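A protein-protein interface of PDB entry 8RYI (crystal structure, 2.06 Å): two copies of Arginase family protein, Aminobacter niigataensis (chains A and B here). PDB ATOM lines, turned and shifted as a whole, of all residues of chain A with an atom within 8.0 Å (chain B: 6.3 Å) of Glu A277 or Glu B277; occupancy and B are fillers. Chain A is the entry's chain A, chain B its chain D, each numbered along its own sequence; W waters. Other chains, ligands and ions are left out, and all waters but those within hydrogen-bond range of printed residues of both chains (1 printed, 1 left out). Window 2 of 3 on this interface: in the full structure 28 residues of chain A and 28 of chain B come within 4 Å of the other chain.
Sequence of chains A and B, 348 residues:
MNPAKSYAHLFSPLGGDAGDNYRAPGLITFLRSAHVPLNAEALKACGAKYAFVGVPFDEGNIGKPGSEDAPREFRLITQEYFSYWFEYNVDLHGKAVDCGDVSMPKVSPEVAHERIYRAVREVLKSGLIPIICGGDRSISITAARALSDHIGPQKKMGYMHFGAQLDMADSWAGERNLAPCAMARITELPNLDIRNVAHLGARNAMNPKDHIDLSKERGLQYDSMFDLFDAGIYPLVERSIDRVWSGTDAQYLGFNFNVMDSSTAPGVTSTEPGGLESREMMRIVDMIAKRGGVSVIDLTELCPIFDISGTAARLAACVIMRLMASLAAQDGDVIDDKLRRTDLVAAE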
ATOM      1  N   ARG A 203      22.959  -5.083  10.463  1.00  0.00           N
ATOM      2  CA  ARG A 203      22.006  -4.128  11.012  1.00  0.00           C
ATOM      3  C   ARG A 203      20.802  -4.884  11.552  1.00  0.00           C
ATOM      4  O   ARG A 203      20.590  -6.052  11.233  1.00  0.00           O
ATOM      5  CB  ARG A 203      21.558  -3.119   9.957  1.00  0.00           C
ATOM      6  CG  ARG A 203      20.850  -3.748   8.745  1.00  0.00           C
ATOM      7  CD  ARG A 203      20.422  -2.685   7.747  1.00  0.00           C
ATOM      8  NE  ARG A 203      19.649  -3.227   6.636  1.00  0.00           N
ATOM      9  CZ  ARG A 203      20.190  -3.785   5.561  1.00  0.00           C
ATOM     10  NH1 ARG A 203      21.509  -3.963   5.458  1.00  0.00           N
ATOM     11  NH2 ARG A 203      19.405  -4.130   4.545  1.00  0.00           N
ATOM     12  N   MET A 225      26.084  -1.529   9.134  1.00  0.00           N
ATOM     13  CA  MET A 225      25.440  -0.538   8.286  1.00  0.00           C
ATOM     14  C   MET A 225      25.549   0.851   8.910  1.00  0.00           C
ATOM     15  O   MET A 225      25.849   1.827   8.210  1.00  0.00           O
ATOM     16  CB  MET A 225      23.980  -0.911   8.042  1.00  0.00           C
ATOM     17  CG  MET A 225      23.390  -0.245   6.830  1.00  0.00           C
ATOM     18  SD  MET A 225      24.112  -0.889   5.286  1.00  0.00           S
ATOM     19  CE  MET A 225      24.802   0.625   4.634  1.00  0.00           C
ATOM     20  N   PHE A 229      27.174   4.056   7.195  1.00  0.00           N
ATOM     21  CA  PHE A 229      26.503   5.346   7.049  1.00  0.00           C
ATOM     22  C   PHE A 229      27.338   6.483   7.639  1.00  0.00           C
ATOM     23  O   PHE A 229      27.500   7.534   7.009  1.00  0.00           O
ATOM     24  CB  PHE A 229      25.124   5.305   7.708  1.00  0.00           C
ATOM     25  CG  PHE A 229      24.105   4.486   6.954  1.00  0.00           C
ATOM     26  CD1 PHE A 229      24.188   4.340   5.584  1.00  0.00           C
ATOM     27  CD2 PHE A 229      23.060   3.869   7.621  1.00  0.00           C
ATOM     28  CE1 PHE A 229      23.240   3.594   4.900  1.00  0.00           C
ATOM     29  CE2 PHE A 229      22.131   3.117   6.941  1.00  0.00           C
ATOM     30  CZ  PHE A 229      22.219   2.979   5.581  1.00  0.00           C
ATOM     31  N   ILE A 233      30.022   5.487   3.707  1.00  0.00           N
ATOM     32  CA  ILE A 233      30.028   4.192   3.019  1.00  0.00           C
ATOM     33  C   ILE A 233      31.375   3.895   2.353  1.00  0.00           C
ATOM     34  O   ILE A 233      32.121   3.016   2.800  1.00  0.00           O
ATOM     35  CB  ILE A 233      28.890   4.098   1.982  1.00  0.00           C
ATOM     36  CG1 ILE A 233      27.520   4.254   2.653  1.00  0.00           C
ATOM     37  CG2 ILE A 233      28.970   2.774   1.226  1.00  0.00           C
ATOM     38  CD1 ILE A 233      26.372   4.180   1.691  1.00  0.00           C
ATOM     39  N   TYR A 234      31.680   4.596   1.264  1.00  0.00           N
ATOM     40  CA  TYR A 234      32.775   4.160   0.400  1.00  0.00           C
ATOM     41  C   TYR A 234      34.154   4.190   1.054  1.00  0.00           C
ATOM     42  O   TYR A 234      34.939   3.265   0.786  1.00  0.00           O
ATOM     43  CB  TYR A 234      32.770   4.986  -0.891  1.00  0.00           C
ATOM     44  CG  TYR A 234      31.394   5.031  -1.529  1.00  0.00           C
ATOM     45  CD1 TYR A 234      30.730   3.860  -1.896  1.00  0.00           C
ATOM     46  CD2 TYR A 234      30.749   6.249  -1.734  1.00  0.00           C
ATOM     47  CE1 TYR A 234      29.465   3.898  -2.465  1.00  0.00           C
ATOM     48  CE2 TYR A 234      29.495   6.306  -2.301  1.00  0.00           C
ATOM     49  CZ  TYR A 234      28.851   5.130  -2.667  1.00  0.00           C
ATOM     50  OH  TYR A 234      27.598   5.213  -3.233  1.00  0.00           O
ATOM     51  N   VAL A 259      21.628  -7.455   2.341  1.00  0.00           N
ATOM     52  CA  VAL A 259      22.474  -6.287   2.582  1.00  0.00           C
ATOM     53  C   VAL A 259      21.837  -5.053   1.959  1.00  0.00           C
ATOM     54  O   VAL A 259      22.020  -3.932   2.451  1.00  0.00           O
ATOM     55  CB  VAL A 259      23.908  -6.516   2.045  1.00  0.00           C
ATOM     56  CG1 VAL A 259      23.955  -6.438   0.517  1.00  0.00           C
ATOM     57  CG2 VAL A 259      24.895  -5.490   2.655  1.00  0.00           C
ATOM     58  N   MET A 260      21.072  -5.235   0.884  1.00  0.00           N
ATOM     59  CA  MET A 260      20.400  -4.118   0.244  1.00  0.00           C
ATOM     60  C   MET A 260      19.174  -3.710   1.051  1.00  0.00           C
ATOM     61  O   MET A 260      18.543  -4.530   1.728  1.00  0.00           O
ATOM     62  CB  MET A 260      19.960  -4.470  -1.178  1.00  0.00           C
ATOM     63  CG  MET A 260      21.014  -5.145  -2.030  1.00  0.00           C
ATOM     64  SD  MET A 260      22.405  -4.043  -2.355  1.00  0.00           S
ATOM     65  CE  MET A 260      21.568  -2.674  -3.190  1.00  0.00           C
ATOM     66  N   ASP A 261      18.834  -2.427   0.946  1.00  0.00           N
ATOM     67  CA  ASP A 261      17.572  -1.921   1.464  1.00  0.00           C
ATOM     68  C   ASP A 261      16.409  -2.762   0.939  1.00  0.00           C
ATOM     69  O   ASP A 261      16.384  -3.149  -0.231  1.00  0.00           O
ATOM     70  CB  ASP A 261      17.394  -0.475   1.022  1.00  0.00           C
ATOM     71  CG  ASP A 261      16.341   0.252   1.813  1.00  0.00           C
ATOM     72  OD1 ASP A 261      16.609   0.613   2.979  1.00  0.00           O
ATOM     73  OD2 ASP A 261      15.227   0.438   1.279  1.00  0.00           O
ATOM     74  N   SER A 262      15.445  -3.048   1.819  1.00  0.00           N
ATOM     75  CA  SER A 262      14.295  -3.883   1.452  1.00  0.00           C
ATOM     76  C   SER A 262      13.651  -3.435   0.144  1.00  0.00           C
ATOM     77  O   SER A 262      13.224  -4.273  -0.658  1.00  0.00           O
ATOM     78  CB  SER A 262      13.240  -3.843   2.565  1.00  0.00           C
ATOM     79  OG  SER A 262      13.606  -4.681   3.638  1.00  0.00           O
ATOM     80  N   SER A 263      13.595  -2.115  -0.097  1.00  0.00           N
ATOM     81  CA  SER A 263      12.941  -1.601  -1.298  1.00  0.00           C
ATOM     82  C   SER A 263      13.554  -2.163  -2.576  1.00  0.00           C
ATOM     83  O   SER A 263      12.829  -2.454  -3.536  1.00  0.00           O
ATOM     84  CB  SER A 263      13.000  -0.065  -1.313  1.00  0.00           C
ATOM     85  OG  SER A 263      14.333   0.402  -1.220  1.00  0.00           O
ATOM     86  N   THR A 264      14.859  -2.406  -2.593  1.00  0.00           N
ATOM     87  CA  THR A 264      15.461  -2.918  -3.807  1.00  0.00           C
ATOM     88  C   THR A 264      15.793  -4.402  -3.711  1.00  0.00           C
ATOM     89  O   THR A 264      16.193  -4.982  -4.714  1.00  0.00           O
ATOM     90  CB  THR A 264      16.713  -2.109  -4.195  1.00  0.00           C
ATOM     91  OG1 THR A 264      17.198  -2.563  -5.472  1.00  0.00           O
ATOM     92  CG2 THR A 264      17.829  -2.237  -3.173  1.00  0.00           C
ATOM     93  N   GLY A 274      16.648  -0.320   5.698  1.00  0.00           N
ATOM     94  CA  GLY A 274      17.758   0.526   6.103  1.00  0.00           C
ATOM     95  C   GLY A 274      19.116   0.076   5.608  1.00  0.00           C
ATOM     96  O   GLY A 274      20.099   0.175   6.347  1.00  0.00           O
ATOM     97  N   GLY A 275      19.189  -0.464   4.391  1.00  0.00           N
ATOM     98  CA  GLY A 275      20.407  -0.980   3.821  1.00  0.00           C
ATOM     99  C   GLY A 275      20.891  -0.184   2.622  1.00  0.00           C
ATOM    100  O   GLY A 275      20.466   0.954   2.380  1.00  0.00           O
ATOM    101  N   LEU A 276      21.789  -0.805   1.854  1.00  0.00           N
ATOM    102  CA  LEU A 276      22.357  -0.197   0.654  1.00  0.00           C
ATOM    103  C   LEU A 276      21.311  -0.025  -0.440  1.00  0.00           C
ATOM    104  O   LEU A 276      20.469  -0.900  -0.661  1.00  0.00           O
ATOM    105  CB  LEU A 276      23.496  -1.067   0.115  1.00  0.00           C
ATOM    106  CG  LEU A 276      24.819  -1.159   0.861  1.00  0.00           C
ATOM    107  CD1 LEU A 276      25.750  -2.175   0.192  1.00  0.00           C
ATOM    108  CD2 LEU A 276      25.463   0.218   0.840  1.00  0.00           C
ATOM    109  N   GLU A 277      21.382   1.093  -1.147  1.00  0.00           N
ATOM    110  CA  GLU A 277      20.560   1.304  -2.326  1.00  0.00           C
ATOM    111  C   GLU A 277      21.351   0.939  -3.579  1.00  0.00           C
ATOM    112  O   GLU A 277      22.576   0.810  -3.547  1.00  0.00           O
ATOM    113  CB  GLU A 277      20.041   2.746  -2.352  1.00  0.00           C
ATOM    114  CG  GLU A 277      18.749   2.847  -1.496  1.00  0.00           C
ATOM    115  CD  GLU A 277      18.529   4.194  -0.817  1.00  0.00           C
ATOM    116  OE1 GLU A 277      19.071   5.217  -1.300  1.00  0.00           O
ATOM    117  OE2 GLU A 277      17.799   4.221   0.211  1.00  0.00           O
ATOM    118  N   SER A 278      20.629   0.718  -4.682  1.00  0.00           N
ATOM    119  CA  SER A 278      21.244   0.038  -5.824  1.00  0.00           C
ATOM    120  C   SER A 278      22.458   0.794  -6.357  1.00  0.00           C
ATOM    121  O   SER A 278      23.471   0.178  -6.681  1.00  0.00           O
ATOM    122  CB  SER A 278      20.240  -0.173  -6.960  1.00  0.00           C
ATOM    123  OG  SER A 278      19.764   1.058  -7.460  1.00  0.00           O
ATOM    124  N   ARG A 279      22.376   2.123  -6.467  1.00  0.00           N
ATOM    125  CA  ARG A 279      23.505   2.876  -7.010  1.00  0.00           C
ATOM    126  C   ARG A 279      24.735   2.754  -6.120  1.00  0.00           C
ATOM    127  O   ARG A 279      25.865   2.825  -6.614  1.00  0.00           O
ATOM    128  CB  ARG A 279      23.149   4.356  -7.177  1.00  0.00           C
ATOM    129  CG  ARG A 279      23.043   5.126  -5.870  1.00  0.00           C
ATOM    130  CD  ARG A 279      22.650   6.589  -6.082  1.00  0.00           C
ATOM    131  NE  ARG A 279      21.294   6.707  -6.613  1.00  0.00           N
ATOM    132  CZ  ARG A 279      20.605   7.843  -6.679  1.00  0.00           C
ATOM    133  NH1 ARG A 279      21.126   8.998  -6.286  1.00  0.00           N
ATOM    134  NH2 ARG A 279      19.353   7.816  -7.127  1.00  0.00           N
ATOM    135  N   GLU A 280      24.536   2.570  -4.811  1.00  0.00           N
ATOM    136  CA  GLU A 280      25.657   2.437  -3.890  1.00  0.00           C
ATOM    137  C   GLU A 280      26.366   1.105  -4.083  1.00  0.00           C
ATOM    138  O   GLU A 280      27.603   1.057  -4.149  1.00  0.00           O
ATOM    139  CB  GLU A 280      25.164   2.587  -2.446  1.00  0.00           C
ATOM    140  CG  GLU A 280      24.728   4.013  -2.066  1.00  0.00           C
ATOM    141  CD  GLU A 280      23.813   4.074  -0.826  1.00  0.00           C
ATOM    142  OE1 GLU A 280      23.182   3.056  -0.485  1.00  0.00           O
ATOM    143  OE2 GLU A 280      23.717   5.154  -0.194  1.00  0.00           O
ATOM    144  N   MET A 281      25.605   0.017  -4.221  1.00  0.00           N
ATOM    145  CA  MET A 281      26.240  -1.269  -4.469  1.00  0.00           C
ATOM    146  C   MET A 281      26.947  -1.273  -5.820  1.00  0.00           C
ATOM    147  O   MET A 281      28.025  -1.867  -5.962  1.00  0.00           O
ATOM    148  CB  MET A 281      25.225  -2.408  -4.374  1.00  0.00           C
ATOM    149  CG  MET A 281      25.843  -3.788  -4.609  1.00  0.00           C
ATOM    150  SD  MET A 281      27.198  -4.254  -3.480  1.00  0.00           S
ATOM    151  CE  MET A 281      26.280  -5.015  -2.156  1.00  0.00           C
ATOM    152  N   MET A 282      26.374  -0.599  -6.827  1.00  0.00           N
ATOM    153  CA  MET A 282      27.042  -0.526  -8.124  1.00  0.00           C
ATOM    154  C   MET A 282      28.398   0.158  -8.009  1.00  0.00           C
ATOM    155  O   MET A 282      29.360  -0.234  -8.684  1.00  0.00           O
ATOM    156  CB  MET A 282      26.163   0.202  -9.139  1.00  0.00           C
ATOM    157  CG  MET A 282      24.843  -0.486  -9.410  1.00  0.00           C
ATOM    158  SD  MET A 282      25.034  -2.269  -9.502  1.00  0.00           S
ATOM    159  CE  MET A 282      23.372  -2.756  -9.949  1.00  0.00           C
ATOM    160  N   ARG A 283      28.499   1.183  -7.150  1.00  0.00           N
ATOM    161  CA  ARG A 283      29.796   1.819  -6.919  1.00  0.00           C
ATOM    162  C   ARG A 283      30.765   0.866  -6.228  1.00  0.00           C
ATOM    163  O   ARG A 283      31.944   0.786  -6.595  1.00  0.00           O
ATOM    164  CB  ARG A 283      29.635   3.074  -6.054  1.00  0.00           C
ATOM    165  CG  ARG A 283      29.265   4.349  -6.786  1.00  0.00           C
ATOM    166  CD  ARG A 283      29.950   5.565  -6.136  1.00  0.00           C
ATOM    167  NE  ARG A 283      31.402   5.402  -6.100  1.00  0.00           N
ATOM    168  CZ  ARG A 283      32.248   6.234  -5.504  1.00  0.00           C
ATOM    169  NH1 ARG A 283      31.822   7.312  -4.856  1.00  0.00           N
ATOM    170  NH2 ARG A 283      33.556   5.978  -5.554  1.00  0.00           N
ATOM    171  N   ILE A 284      30.274   0.131  -5.234  1.00  0.00           N
ATOM    172  CA  ILE A 284      31.091  -0.836  -4.511  1.00  0.00           C
ATOM    173  C   ILE A 284      31.626  -1.913  -5.447  1.00  0.00           C
ATOM    174  O   ILE A 284      32.777  -2.347  -5.320  1.00  0.00           O
ATOM    175  CB  ILE A 284      30.268  -1.429  -3.358  1.00  0.00           C
ATOM    176  CG1 ILE A 284      30.075  -0.357  -2.279  1.00  0.00           C
ATOM    177  CG2 ILE A 284      30.878  -2.737  -2.844  1.00  0.00           C
ATOM    178  CD1 ILE A 284      29.082  -0.736  -1.219  1.00  0.00           C
ATOM    179  N   LEU A 315      18.040  -7.083  -9.400  1.00  0.00           N
ATOM    180  CA  LEU A 315      19.159  -6.377  -8.782  1.00  0.00           C
ATOM    181  C   LEU A 315      20.361  -7.301  -8.660  1.00  0.00           C
ATOM    182  O   LEU A 315      21.490  -6.929  -9.000  1.00  0.00           O
ATOM    183  CB  LEU A 315      18.789  -5.843  -7.396  1.00  0.00           C
ATOM    184  CG  LEU A 315      20.083  -5.222  -6.850  1.00  0.00           C
ATOM    185  CD1 LEU A 315      20.324  -3.741  -7.269  1.00  0.00           C
ATOM    186  CD2 LEU A 315      20.275  -5.428  -5.384  1.00  0.00           C
ATOM    187  N   VAL A 319      24.032  -6.794 -10.468  1.00  0.00           N
ATOM    188  CA  VAL A 319      25.281  -6.680  -9.717  1.00  0.00           C
ATOM    189  C   VAL A 319      26.315  -7.680 -10.230  1.00  0.00           C
ATOM    190  O   VAL A 319      27.493  -7.347 -10.396  1.00  0.00           O
ATOM    191  CB  VAL A 319      25.008  -6.850  -8.211  1.00  0.00           C
ATOM    192  CG1 VAL A 319      26.308  -7.023  -7.429  1.00  0.00           C
ATOM    193  CG2 VAL A 319      24.204  -5.669  -7.700  1.00  0.00           C
ATOM    194  N   VAL B 259      13.612   5.235 -16.408  1.00  0.00           N
ATOM    195  CA  VAL B 259      14.649   6.127 -15.899  1.00  0.00           C
ATOM    196  C   VAL B 259      14.729   6.028 -14.379  1.00  0.00           C
ATOM    197  O   VAL B 259      15.798   6.244 -13.792  1.00  0.00           O
ATOM    198  CB  VAL B 259      14.394   7.579 -16.362  1.00  0.00           C
ATOM    199  CG1 VAL B 259      13.218   8.207 -15.587  1.00  0.00           C
ATOM    200  CG2 VAL B 259      15.665   8.427 -16.215  1.00  0.00           C
ATOM    201  N   MET B 260      13.611   5.696 -13.719  1.00  0.00           N
ATOM    202  CA  MET B 260      13.585   5.571 -12.268  1.00  0.00           C
ATOM    203  C   MET B 260      14.191   4.243 -11.836  1.00  0.00           C
ATOM    204  O   MET B 260      14.156   3.257 -12.576  1.00  0.00           O
ATOM    205  CB  MET B 260      12.158   5.656 -11.728  1.00  0.00           C
ATOM    206  CG  MET B 260      11.324   6.761 -12.295  1.00  0.00           C
ATOM    207  SD  MET B 260      11.988   8.379 -11.874  1.00  0.00           S
ATOM    208  CE  MET B 260      11.983   8.327 -10.073  1.00  0.00           C
ATOM    209  N   ASP B 261      14.746   4.225 -10.621  1.00  0.00           N
ATOM    210  CA  ASP B 261      15.190   2.978 -10.016  1.00  0.00           C
ATOM    211  C   ASP B 261      14.050   1.964  -9.988  1.00  0.00           C
ATOM    212  O   ASP B 261      12.906   2.297  -9.652  1.00  0.00           O
ATOM    213  CB  ASP B 261      15.704   3.244  -8.599  1.00  0.00           C
ATOM    214  CG  ASP B 261      16.523   2.096  -8.053  1.00  0.00           C
ATOM    215  OD1 ASP B 261      17.643   1.888  -8.546  1.00  0.00           O
ATOM    216  OD2 ASP B 261      16.075   1.419  -7.108  1.00  0.00           O
ATOM    217  N   THR B 264      11.191   1.839  -7.427  1.00  0.00           N
ATOM    218  CA  THR B 264      10.107   2.801  -7.382  1.00  0.00           C
ATOM    219  C   THR B 264       9.298   2.868  -8.673  1.00  0.00           C
ATOM    220  O   THR B 264       8.372   3.682  -8.762  1.00  0.00           O
ATOM    221  CB  THR B 264      10.640   4.197  -7.018  1.00  0.00           C
ATOM    222  OG1 THR B 264       9.526   5.056  -6.721  1.00  0.00           O
ATOM    223  CG2 THR B 264      11.392   4.794  -8.165  1.00  0.00           C
ATOM    224  N   GLY B 275      18.588   3.640 -10.982  1.00  0.00           N
ATOM    225  CA  GLY B 275      18.028   4.817 -11.599  1.00  0.00           C
ATOM    226  C   GLY B 275      17.705   5.913 -10.598  1.00  0.00           C
ATOM    227  O   GLY B 275      18.154   5.906  -9.449  1.00  0.00           O
ATOM    228  N   LEU B 276      16.908   6.875 -11.066  1.00  0.00           N
ATOM    229  CA  LEU B 276      16.528   8.021 -10.246  1.00  0.00           C
ATOM    230  C   LEU B 276      15.617   7.620  -9.091  1.00  0.00           C
ATOM    231  O   LEU B 276      14.768   6.725  -9.217  1.00  0.00           O
ATOM    232  CB  LEU B 276      15.802   9.072 -11.084  1.00  0.00           C
ATOM    233  CG  LEU B 276      16.634   9.808 -12.116  1.00  0.00           C
ATOM    234  CD1 LEU B 276      15.747  10.767 -12.884  1.00  0.00           C
ATOM    235  CD2 LEU B 276      17.793  10.508 -11.440  1.00  0.00           C
ATOM    236  N   GLU B 277      15.774   8.330  -7.969  1.00  0.00           N
ATOM    237  CA  GLU B 277      14.800   8.277  -6.884  1.00  0.00           C
ATOM    238  C   GLU B 277      13.630   9.213  -7.181  1.00  0.00           C
ATOM    239  O   GLU B 277      13.748  10.181  -7.938  1.00  0.00           O
ATOM    240  CB  GLU B 277      15.451   8.655  -5.555  1.00  0.00           C
ATOM    241  CG  GLU B 277      16.632   7.755  -5.172  1.00  0.00           C
ATOM    242  CD  GLU B 277      17.454   8.300  -4.009  1.00  0.00           C
ATOM    243  OE1 GLU B 277      16.949   9.166  -3.268  1.00  0.00           O
ATOM    244  OE2 GLU B 277      18.611   7.869  -3.827  1.00  0.00           O
ATOM    245  N   SER B 278      12.479   8.909  -6.580  1.00  0.00           N
ATOM    246  CA  SER B 278      11.313   9.763  -6.784  1.00  0.00           C
ATOM    247  C   SER B 278      11.605  11.207  -6.364  1.00  0.00           C
ATOM    248  O   SER B 278      11.213  12.154  -7.054  1.00  0.00           O
ATOM    249  CB  SER B 278      10.097   9.181  -6.045  1.00  0.00           C
ATOM    250  OG  SER B 278      10.334   9.053  -4.645  1.00  0.00           O
ATOM    251  N   ARG B 279      12.303  11.396  -5.241  1.00  0.00           N
ATOM    252  CA  ARG B 279      12.601  12.760  -4.803  1.00  0.00           C
ATOM    253  C   ARG B 279      13.491  13.479  -5.793  1.00  0.00           C
ATOM    254  O   ARG B 279      13.424  14.713  -5.912  1.00  0.00           O
ATOM    255  CB  ARG B 279      13.238  12.764  -3.419  1.00  0.00           C
ATOM    256  CG  ARG B 279      14.577  12.079  -3.323  1.00  0.00           C
ATOM    257  CD  ARG B 279      15.130  12.220  -1.917  1.00  0.00           C
ATOM    258  NE  ARG B 279      14.236  11.638  -0.918  1.00  0.00           N
ATOM    259  CZ  ARG B 279      14.579  11.420   0.344  1.00  0.00           C
ATOM    260  NH1 ARG B 279      15.794  11.716   0.798  1.00  0.00           N
ATOM    261  NH2 ARG B 279      13.682  10.894   1.178  1.00  0.00           N
ATOM    262  N   GLU B 280      14.338  12.739  -6.504  1.00  0.00           N
ATOM    263  CA  GLU B 280      15.171  13.392  -7.498  1.00  0.00           C
ATOM    264  C   GLU B 280      14.326  13.830  -8.686  1.00  0.00           C
ATOM    265  O   GLU B 280      14.470  14.965  -9.163  1.00  0.00           O
ATOM    266  CB  GLU B 280      16.324  12.468  -7.909  1.00  0.00           C
ATOM    267  CG  GLU B 280      17.341  12.253  -6.775  1.00  0.00           C
ATOM    268  CD  GLU B 280      18.237  11.049  -6.965  1.00  0.00           C
ATOM    269  OE1 GLU B 280      17.885  10.131  -7.745  1.00  0.00           O
ATOM    270  OE2 GLU B 280      19.317  11.020  -6.336  1.00  0.00           O
ATOM    271  N   MET B 281      13.393  12.976  -9.138  1.00  0.00           N
ATOM    272  CA  MET B 281      12.538  13.371 -10.256  1.00  0.00           C
ATOM    273  C   MET B 281      11.626  14.539  -9.895  1.00  0.00           C
ATOM    274  O   MET B 281      11.326  15.369 -10.763  1.00  0.00           O
ATOM    275  CB  MET B 281      11.717  12.189 -10.757  1.00  0.00           C
ATOM    276  CG  MET B 281      10.813  12.516 -11.953  1.00  0.00           C
ATOM    277  SD  MET B 281      11.696  13.179 -13.398  1.00  0.00           S
ATOM    278  CE  MET B 281      12.200  11.676 -14.227  1.00  0.00           C
ATOM    279  N   MET B 282      11.190  14.646  -8.634  1.00  0.00           N
ATOM    280  CA  MET B 282      10.335  15.774  -8.268  1.00  0.00           C
ATOM    281  C   MET B 282      11.096  17.101  -8.373  1.00  0.00           C
ATOM    282  O   MET B 282      10.581  18.075  -8.929  1.00  0.00           O
ATOM    283  CB  MET B 282       9.754  15.579  -6.864  1.00  0.00           C
ATOM    284  CG  MET B 282       8.849  14.341  -6.729  1.00  0.00           C
ATOM    285  SD  MET B 282       7.805  14.150  -8.196  1.00  0.00           S
ATOM    286  CE  MET B 282       7.097  12.511  -7.907  1.00  0.00           C
ATOM    287  N   LEU B 315       3.557   6.832  -9.475  1.00  0.00           N
ATOM    288  CA  LEU B 315       4.708   7.695  -9.666  1.00  0.00           C
ATOM    289  C   LEU B 315       4.560   8.556 -10.916  1.00  0.00           C
ATOM    290  O   LEU B 315       4.770   9.767 -10.861  1.00  0.00           O
ATOM    291  CB  LEU B 315       5.985   6.861  -9.725  1.00  0.00           C
ATOM    292  CG  LEU B 315       7.123   7.849  -9.994  1.00  0.00           C
ATOM    293  CD1 LEU B 315       7.577   8.501  -8.687  1.00  0.00           C
ATOM    294  CD2 LEU B 315       8.248   7.157 -10.656  1.00  0.00           C
HETATM  295  O   HOH W   1      17.955   1.100  -4.673  1.00  0.00           O
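Thr A264 touches none of the printed residues of chain B.
Printed residues of chain B within 4 Å of Ser A278: Asp B261.
Printed residues of chain B within 4 Å of Arg A279: Gly B275, Glu B277 and Glu B280.
Of the printed residues of chain A, Asp B261 touches Ser A278 (2.5 Å).
Glu B277 touches just these residues of chain A: Glu A277 (3.7 Å) and Arg A279 (3.4 Å).
Printed residues of chain A within 4 Å of Glu B280: Arg A279.
Met B282 touches none of the printed residues of chain A.
The nearest residue of chain A that does not touch Glu B277 is Glu A280 (6.8 Å).
The nearest printed residue of chain B that does not touch Ser A278 is Gly B275 (4.5 Å).
Glu B277 touches Glu A277 (OE2 to OE1, 3.7 Å).
Glu B277 touches its own counterpart, Glu A277.
Ser A278 touches Asp B261, but with the chains exchanged Asp A261 does not touch Ser B278 (11.5 Å).
Arg A279 touches Glu B277, but with the chains exchanged Glu A277 does not touch Arg B279 (7.6 Å).
Arg A279 touches Glu B280, but with the chains exchanged Glu A280 does not touch Arg B279 (10.3 Å).
Water W1 bridges N of Ser A278 (2.7 Å) and OD2 of Asp B261 (3.1 Å).
The backbone NH of Gly B275 sits at hydrogen-bond distance from the side-chain carboxylate of Asp B261 (3.1 Å).
The backbone NH (N) of Asp B261 lies within hydrogen-bond range of the backbone carbonyl oxygen (O) of Leu B276, 2.9 Å away.
N of Glu B277 sits at hydrogen-bond distance from OE1 of Glu B280, at 2.8 Å.
The side-chain carboxylate (OE1) of Glu A280 lies within hydrogen-bond range of the backbone NH (N) of Glu A277 (2.7 Å).
Among the printed residues, Asp or Glu carboxylates within 4 Å of a Lys or Arg side-chain nitrogen of the other chain: Arg A279 with Glu B277 (3.4 Å) and Arg A279 with Glu B280 (2.7 Å).
The side-chain hydroxyl of Ser A278 sits at hydrogen-bond distance from the side-chain carboxylate of Asp B261.
The side-chain carboxylate (OE2) of Glu B280 lies within salt-bridge range of the guanidinium group (NH1) of Arg A279, at 2.7 Å.
The backbone carbonyl oxygen (O) of Gly B275 sits at hydrogen-bond distance from the guanidinium group (NH2) of Arg A279 (3.2 Å).
The guanidinium group (NH2) of Arg A279 lies within salt-bridge range of the side-chain carboxylate (OE2) of Glu B277 (3.4 Å).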
